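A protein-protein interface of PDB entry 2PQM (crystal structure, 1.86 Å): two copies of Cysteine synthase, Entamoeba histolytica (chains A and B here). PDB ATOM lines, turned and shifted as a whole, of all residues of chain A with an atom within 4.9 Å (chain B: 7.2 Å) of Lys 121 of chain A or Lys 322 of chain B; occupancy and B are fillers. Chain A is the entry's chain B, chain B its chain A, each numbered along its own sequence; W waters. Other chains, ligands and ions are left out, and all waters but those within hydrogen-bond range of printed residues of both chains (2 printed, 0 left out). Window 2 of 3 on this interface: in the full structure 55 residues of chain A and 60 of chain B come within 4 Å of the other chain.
Hydrophobic or aromatic side chains of chain A that line the printed part of chain B: Ala 122 and Phe 123. Along chain A the printed residues that touch a printed residue of chain B span positions 121 to 123. Among the printed residues, 4 pairs touch across the chains. Among the printed residues, no Asp or Glu carboxylate lies within 4 Å of a Lys or Arg side-chain nitrogen of the other chain.
No position is printed for both chains. Of the 4 pairs that touch across the chains among the printed residues, none has its exchanged pair printed and touching as well.
Lys 322 of chain B touches one residue of chain A. Of the printed residues of chain A, Tyr 319 of chain B touches Ala 122. Of the printed residues of chain B, Ala 122 of chain A touches Val 270 (3.2 Å) and Tyr 319 (3.5 Å). Of the printed residues of chain B, Phe 123 of chain A touches Val 270 (3.6 Å). Gly 124 of chain A touches none of the printed residues of chain B. Lys 320 of chain B touches none of the printed residues of chain A. The nearest residue of chain B that does not touch Lys 121 of chain A is Lys 271 of chain B (6.4 Å). The nearest residue of chain A that does not touch Lys 322 of chain B is Ala 122 of chain A (4.8 Å).
The backbone carbonyl oxygen of Tyr 319 of chain B is in hydrogen-bond range of the side-chain amino group of Lys 322 of chain B (2.9 Å).
Water W1 bridges the backbone carbonyl oxygen (O) of Lys 271 of chain B (2.6 Å) and the backbone carbonyl oxygen (O) of Phe 123 of chain A (2.8 Å). Water W2 bridges the backbone carbonyl oxygen (O) of Ala 122 of chain A (2.7 Å) and the backbone carbonyl oxygen (O) of Arg 267 of chain B (2.8 Å).
CE of Lys 121 of chain A touches CE of Lys 322 of chain B, 3.9 Å away. Ala 122 of chain A touches Val 270 of chain B (O to CG1, 3.2 Å). CB of Ala 122 of chain A touches CD1 of Tyr 319 of chain B, at 3.5 Å. CG2 of Val 270 of chain B touches CE1 of Phe 123 of chain A, at 3.6 Å.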
ATOM      1  N   GLN A 117     -12.534  -2.590 -10.707  1.00  0.00           N
ATOM      2  CA  GLN A 117     -13.265  -3.820 -10.988  1.00  0.00           C
ATOM      3  C   GLN A 117     -12.706  -4.541 -12.196  1.00  0.00           C
ATOM      4  O   GLN A 117     -12.466  -5.740 -12.146  1.00  0.00           O
ATOM      5  CB  GLN A 117     -14.740  -3.542 -11.236  1.00  0.00           C
ATOM      6  CG  GLN A 117     -15.558  -3.512  -9.968  1.00  0.00           C
ATOM      7  CD  GLN A 117     -16.984  -3.119 -10.230  1.00  0.00           C
ATOM      8  OE1 GLN A 117     -17.635  -3.649 -11.144  1.00  0.00           O
ATOM      9  NE2 GLN A 117     -17.487  -2.177  -9.434  1.00  0.00           N
ATOM     10  N   MET A 118     -12.525  -3.804 -13.290  1.00  0.00           N
ATOM     11  CA  MET A 118     -11.958  -4.399 -14.496  1.00  0.00           C
ATOM     12  C   MET A 118     -10.551  -4.938 -14.236  1.00  0.00           C
ATOM     13  O   MET A 118     -10.219  -6.021 -14.708  1.00  0.00           O
ATOM     14  CB  MET A 118     -11.918  -3.392 -15.638  1.00  0.00           C
ATOM     15  CG  MET A 118     -11.416  -4.001 -16.953  1.00  0.00           C
ATOM     16  SD  MET A 118     -11.260  -2.789 -18.285  1.00  0.00           S
ATOM     17  CE  MET A 118     -12.764  -1.811 -17.971  1.00  0.00           C
ATOM     18  N   ILE A 119      -9.732  -4.174 -13.504  1.00  0.00           N
ATOM     19  CA  ILE A 119      -8.365  -4.631 -13.158  1.00  0.00           C
ATOM     20  C   ILE A 119      -8.473  -5.953 -12.422  1.00  0.00           C
ATOM     21  O   ILE A 119      -7.833  -6.936 -12.783  1.00  0.00           O
ATOM     22  CB  ILE A 119      -7.577  -3.611 -12.308  1.00  0.00           C
ATOM     23  CG1 ILE A 119      -7.383  -2.297 -13.097  1.00  0.00           C
ATOM     24  CG2 ILE A 119      -6.204  -4.223 -11.839  1.00  0.00           C
ATOM     25  CD1 ILE A 119      -6.702  -1.176 -12.299  1.00  0.00           C
ATOM     26  N   MET A 120      -9.314  -5.990 -11.406  1.00  0.00           N
ATOM     27  CA  MET A 120      -9.437  -7.218 -10.623  1.00  0.00           C
ATOM     28  C   MET A 120      -9.921  -8.415 -11.451  1.00  0.00           C
ATOM     29  O   MET A 120      -9.355  -9.506 -11.352  1.00  0.00           O
ATOM     30  CB  MET A 120     -10.201  -6.961  -9.333  1.00  0.00           C
ATOM     31  CG  MET A 120      -9.380  -5.988  -8.379  1.00  0.00           C
ATOM     32  SD  MET A 120     -10.279  -5.756  -6.878  1.00  0.00           S
ATOM     33  CE  MET A 120     -10.210  -3.980  -6.632  1.00  0.00           C
ATOM     34  N   LYS A 121     -10.908  -8.198 -12.321  1.00  0.00           N
ATOM     35  CA  LYS A 121     -11.369  -9.265 -13.231  1.00  0.00           C
ATOM     36  C   LYS A 121     -10.265  -9.729 -14.191  1.00  0.00           C
ATOM     37  O   LYS A 121     -10.142 -10.929 -14.446  1.00  0.00           O
ATOM     38  CB  LYS A 121     -12.608  -8.840 -14.048  1.00  0.00           C
ATOM     39  CG  LYS A 121     -13.893  -8.686 -13.226  1.00  0.00           C
ATOM     40  CD  LYS A 121     -15.070  -8.208 -14.110  1.00  0.00           C
ATOM     41  CE  LYS A 121     -15.817  -9.394 -14.719  1.00  0.00           C
ATOM     42  NZ  LYS A 121     -16.989  -8.977 -15.580  1.00  0.00           N
ATOM     43  N   ALA A 122      -9.458  -8.787 -14.689  1.00  0.00           N
ATOM     44  CA  ALA A 122      -8.343  -9.126 -15.592  1.00  0.00           C
ATOM     45  C   ALA A 122      -7.394 -10.144 -14.937  1.00  0.00           C
ATOM     46  O   ALA A 122      -6.849 -11.017 -15.609  1.00  0.00           O
ATOM     47  CB  ALA A 122      -7.595  -7.835 -16.041  1.00  0.00           C
ATOM     48  N   PHE A 123      -7.217 -10.049 -13.613  1.00  0.00           N
ATOM     49  CA  PHE A 123      -6.396 -11.008 -12.858  1.00  0.00           C
ATOM     50  C   PHE A 123      -7.094 -12.330 -12.538  1.00  0.00           C
ATOM     51  O   PHE A 123      -6.502 -13.206 -11.921  1.00  0.00           O
ATOM     52  CB  PHE A 123      -5.915 -10.383 -11.542  1.00  0.00           C
ATOM     53  CG  PHE A 123      -4.702  -9.505 -11.695  1.00  0.00           C
ATOM     54  CD1 PHE A 123      -3.411 -10.037 -11.536  1.00  0.00           C
ATOM     55  CD2 PHE A 123      -4.848  -8.154 -11.980  1.00  0.00           C
ATOM     56  CE1 PHE A 123      -2.289  -9.210 -11.663  1.00  0.00           C
ATOM     57  CE2 PHE A 123      -3.722  -7.312 -12.113  1.00  0.00           C
ATOM     58  CZ  PHE A 123      -2.451  -7.842 -11.958  1.00  0.00           C
ATOM     59  N   GLY A 124      -8.349 -12.453 -12.940  1.00  0.00           N
ATOM     60  CA  GLY A 124      -9.094 -13.690 -12.764  1.00  0.00           C
ATOM     61  C   GLY A 124      -9.900 -13.724 -11.478  1.00  0.00           C
ATOM     62  O   GLY A 124     -10.394 -14.792 -11.081  1.00  0.00           O
ATOM     63  N   ALA A 125     -10.068 -12.565 -10.846  1.00  0.00           N
ATOM     64  CA  ALA A 125     -10.839 -12.502  -9.606  1.00  0.00           C
ATOM     65  C   ALA A 125     -12.321 -12.714  -9.871  1.00  0.00           C
ATOM     66  O   ALA A 125     -12.855 -12.295 -10.920  1.00  0.00           O
ATOM     67  CB  ALA A 125     -10.627 -11.189  -8.884  1.00  0.00           C
ATOM     68  N   LEU A 127     -15.664 -11.247  -8.647  1.00  0.00           N
ATOM     69  CA  LEU A 127     -16.175 -10.070  -7.952  1.00  0.00           C
ATOM     70  C   LEU A 127     -17.533 -10.302  -7.311  1.00  0.00           C
ATOM     71  O   LEU A 127     -18.444 -10.827  -7.954  1.00  0.00           O
ATOM     72  CB  LEU A 127     -16.279  -8.888  -8.898  1.00  0.00           C
ATOM     73  CG  LEU A 127     -14.987  -8.320  -9.497  1.00  0.00           C
ATOM     74  CD1 LEU A 127     -15.292  -6.938 -10.011  1.00  0.00           C
ATOM     75  CD2 LEU A 127     -13.807  -8.297  -8.500  1.00  0.00           C
ATOM     76  N   ARG B 267      -4.206 -11.031 -22.047  1.00  0.00           N
ATOM     77  CA  ARG B 267      -5.171 -11.515 -21.055  1.00  0.00           C
ATOM     78  C   ARG B 267      -4.646 -12.757 -20.357  1.00  0.00           C
ATOM     79  O   ARG B 267      -4.813 -12.909 -19.130  1.00  0.00           O
ATOM     80  CB  ARG B 267      -6.554 -11.766 -21.693  1.00  0.00           C
ATOM     81  CG  ARG B 267      -7.311 -10.507 -22.043  1.00  0.00           C
ATOM     82  CD  ARG B 267      -8.779 -10.801 -22.417  1.00  0.00           C
ATOM     83  NE  ARG B 267      -8.949 -11.785 -23.512  1.00  0.00           N
ATOM     84  CZ  ARG B 267      -9.031 -11.473 -24.805  1.00  0.00           C
ATOM     85  NH1 ARG B 267      -8.916 -10.210 -25.192  1.00  0.00           N
ATOM     86  NH2 ARG B 267      -9.233 -12.438 -25.718  1.00  0.00           N
ATOM     87  N   VAL B 270      -1.617 -11.917 -17.782  1.00  0.00           N
ATOM     88  CA  VAL B 270      -2.036 -11.394 -16.475  1.00  0.00           C
ATOM     89  C   VAL B 270      -2.717 -12.460 -15.618  1.00  0.00           C
ATOM     90  O   VAL B 270      -2.453 -12.581 -14.412  1.00  0.00           O
ATOM     91  CB  VAL B 270      -2.856 -10.063 -16.587  1.00  0.00           C
ATOM     92  CG1 VAL B 270      -4.198 -10.259 -17.297  1.00  0.00           C
ATOM     93  CG2 VAL B 270      -3.054  -9.426 -15.220  1.00  0.00           C
ATOM     94  N   LYS B 271      -3.541 -13.292 -16.251  1.00  0.00           N
ATOM     95  CA  LYS B 271      -4.282 -14.315 -15.490  1.00  0.00           C
ATOM     96  C   LYS B 271      -3.390 -15.455 -14.988  1.00  0.00           C
ATOM     97  O   LYS B 271      -3.581 -15.941 -13.858  1.00  0.00           O
ATOM     98  CB  LYS B 271      -5.452 -14.821 -16.345  1.00  0.00           C
ATOM     99  CG  LYS B 271      -6.257 -15.964 -15.756  1.00  0.00           C
ATOM    100  CD  LYS B 271      -7.498 -16.264 -16.655  1.00  0.00           C
ATOM    101  CE  LYS B 271      -8.538 -17.071 -15.890  1.00  0.00           C
ATOM    102  NZ  LYS B 271      -9.629 -17.560 -16.777  1.00  0.00           N
ATOM    103  N   LEU B 318      -9.410  -4.472 -24.628  1.00  0.00           N
ATOM    104  CA  LEU B 318      -8.426  -5.486 -24.196  1.00  0.00           C
ATOM    105  C   LEU B 318      -9.039  -6.518 -23.242  1.00  0.00           C
ATOM    106  O   LEU B 318      -8.870  -7.721 -23.454  1.00  0.00           O
ATOM    107  CB  LEU B 318      -7.177  -4.827 -23.566  1.00  0.00           C
ATOM    108  CG  LEU B 318      -6.069  -5.712 -22.969  1.00  0.00           C
ATOM    109  CD1 LEU B 318      -5.591  -6.714 -24.024  1.00  0.00           C
ATOM    110  CD2 LEU B 318      -4.904  -4.836 -22.451  1.00  0.00           C
ATOM    111  N   TYR B 319      -9.719  -6.056 -22.190  1.00  0.00           N
ATOM    112  CA  TYR B 319     -10.253  -6.978 -21.193  1.00  0.00           C
ATOM    113  C   TYR B 319     -11.753  -7.186 -21.295  1.00  0.00           C
ATOM    114  O   TYR B 319     -12.355  -7.781 -20.411  1.00  0.00           O
ATOM    115  CB  TYR B 319      -9.893  -6.556 -19.745  1.00  0.00           C
ATOM    116  CG  TYR B 319      -8.406  -6.368 -19.523  1.00  0.00           C
ATOM    117  CD1 TYR B 319      -7.536  -7.456 -19.545  1.00  0.00           C
ATOM    118  CD2 TYR B 319      -7.872  -5.092 -19.332  1.00  0.00           C
ATOM    119  CE1 TYR B 319      -6.159  -7.293 -19.366  1.00  0.00           C
ATOM    120  CE2 TYR B 319      -6.489  -4.912 -19.146  1.00  0.00           C
ATOM    121  CZ  TYR B 319      -5.647  -6.030 -19.166  1.00  0.00           C
ATOM    122  OH  TYR B 319      -4.294  -5.890 -18.997  1.00  0.00           O
ATOM    123  N   LYS B 320     -12.362  -6.703 -22.368  1.00  0.00           N
ATOM    124  CA  LYS B 320     -13.799  -6.856 -22.502  1.00  0.00           C
ATOM    125  C   LYS B 320     -14.183  -8.286 -22.958  1.00  0.00           C
ATOM    126  O   LYS B 320     -15.130  -8.885 -22.419  1.00  0.00           O
ATOM    127  CB  LYS B 320     -14.396  -5.677 -23.302  1.00  0.00           C
ATOM    128  CG  LYS B 320     -14.075  -4.309 -22.628  1.00  0.00           C
ATOM    129  CD  LYS B 320     -15.095  -3.214 -22.936  1.00  0.00           C
ATOM    130  CE  LYS B 320     -14.446  -1.848 -23.179  1.00  0.00           C
ATOM    131  NZ  LYS B 320     -14.019  -1.094 -21.937  1.00  0.00           N
ATOM    132  N   ILE B 321     -13.400  -8.864 -23.865  1.00  0.00           N
ATOM    133  CA  ILE B 321     -13.543 -10.269 -24.261  1.00  0.00           C
ATOM    134  C   ILE B 321     -13.092 -11.197 -23.123  1.00  0.00           C
ATOM    135  O   ILE B 321     -11.967 -11.063 -22.621  1.00  0.00           O
ATOM    136  CB  ILE B 321     -12.720 -10.549 -25.565  1.00  0.00           C
ATOM    137  CG1 ILE B 321     -12.588  -9.267 -26.403  1.00  0.00           C
ATOM    138  CG2 ILE B 321     -13.309 -11.658 -26.368  1.00  0.00           C
ATOM    139  CD1 ILE B 321     -11.281  -8.520 -26.151  1.00  0.00           C
ATOM    140  N   LYS B 322     -13.967 -12.104 -22.683  1.00  0.00           N
ATOM    141  CA  LYS B 322     -13.658 -12.993 -21.543  1.00  0.00           C
ATOM    142  C   LYS B 322     -13.499 -14.466 -21.938  1.00  0.00           C
ATOM    143  O   LYS B 322     -14.495 -15.200 -22.108  1.00  0.00           O
ATOM    144  CB  LYS B 322     -14.693 -12.851 -20.422  1.00  0.00           C
ATOM    145  CG  LYS B 322     -14.505 -11.608 -19.532  1.00  0.00           C
ATOM    146  CD  LYS B 322     -13.445 -11.819 -18.431  1.00  0.00           C
ATOM    147  CE  LYS B 322     -13.392 -10.643 -17.440  1.00  0.00           C
ATOM    148  NZ  LYS B 322     -12.821  -9.376 -18.005  1.00  0.00           N
ATOM    149  N   ASP B 323     -12.244 -14.894 -22.062  1.00  0.00           N
ATOM    150  CA  ASP B 323     -11.904 -16.162 -22.714  1.00  0.00           C
ATOM    151  C   ASP B 323     -12.522 -17.363 -22.016  1.00  0.00           C
ATOM    152  O   ASP B 323     -12.364 -17.538 -20.803  1.00  0.00           O
ATOM    153  CB  ASP B 323     -10.383 -16.331 -22.809  1.00  0.00           C
ATOM    154  CG  ASP B 323      -9.729 -15.221 -23.610  1.00  0.00           C
ATOM    155  OD1 ASP B 323     -10.056 -15.081 -24.812  1.00  0.00           O
ATOM    156  OD2 ASP B 323      -8.910 -14.472 -23.020  1.00  0.00           O
ATOM    157  N   GLU B 324     -13.222 -18.190 -22.791  1.00  0.00           N
ATOM    158  CA  GLU B 324     -13.733 -19.451 -22.262  1.00  0.00           C
ATOM    159  C   GLU B 324     -12.638 -20.493 -22.391  1.00  0.00           C
ATOM    160  O   GLU B 324     -11.950 -20.568 -23.408  1.00  0.00           O
ATOM    161  CB  GLU B 324     -14.962 -19.926 -23.042  1.00  0.00           C
ATOM    162  CG  GLU B 324     -16.016 -18.867 -23.329  1.00  0.00           C
ATOM    163  CD  GLU B 324     -16.812 -19.171 -24.597  1.00  0.00           C
ATOM    164  OE1 GLU B 324     -16.230 -19.742 -25.557  1.00  0.00           O
ATOM    165  OE2 GLU B 324     -18.017 -18.828 -24.640  1.00  0.00           O
ATOM    166  N   GLY B 325     -12.466 -21.309 -21.371  1.00  0.00           N
ATOM    167  CA  GLY B 325     -11.485 -22.357 -21.489  1.00  0.00           C
ATOM    168  C   GLY B 325     -10.452 -22.341 -20.405  1.00  0.00           C
ATOM    169  O   GLY B 325     -10.193 -21.322 -19.753  1.00  0.00           O
ATOM    170  N   ILE B 330      -6.393 -22.257 -23.762  1.00  0.00           N
ATOM    171  CA  ILE B 330      -6.104 -20.886 -24.188  1.00  0.00           C
ATOM    172  C   ILE B 330      -4.713 -20.863 -24.840  1.00  0.00           C
ATOM    173  O   ILE B 330      -4.569 -20.358 -25.943  1.00  0.00           O
ATOM    174  CB  ILE B 330      -6.307 -19.862 -23.012  1.00  0.00           C
ATOM    175  CG1 ILE B 330      -7.815 -19.589 -22.799  1.00  0.00           C
ATOM    176  CG2 ILE B 330      -5.589 -18.517 -23.317  1.00  0.00           C
ATOM    177  CD1 ILE B 330      -8.157 -18.922 -21.426  1.00  0.00           C
HETATM  178  O   HOH W   1      -5.592 -15.800 -12.171  1.00  0.00           O
HETATM  179  O   HOH W   2      -7.146 -11.533 -18.276  1.00  0.00           O
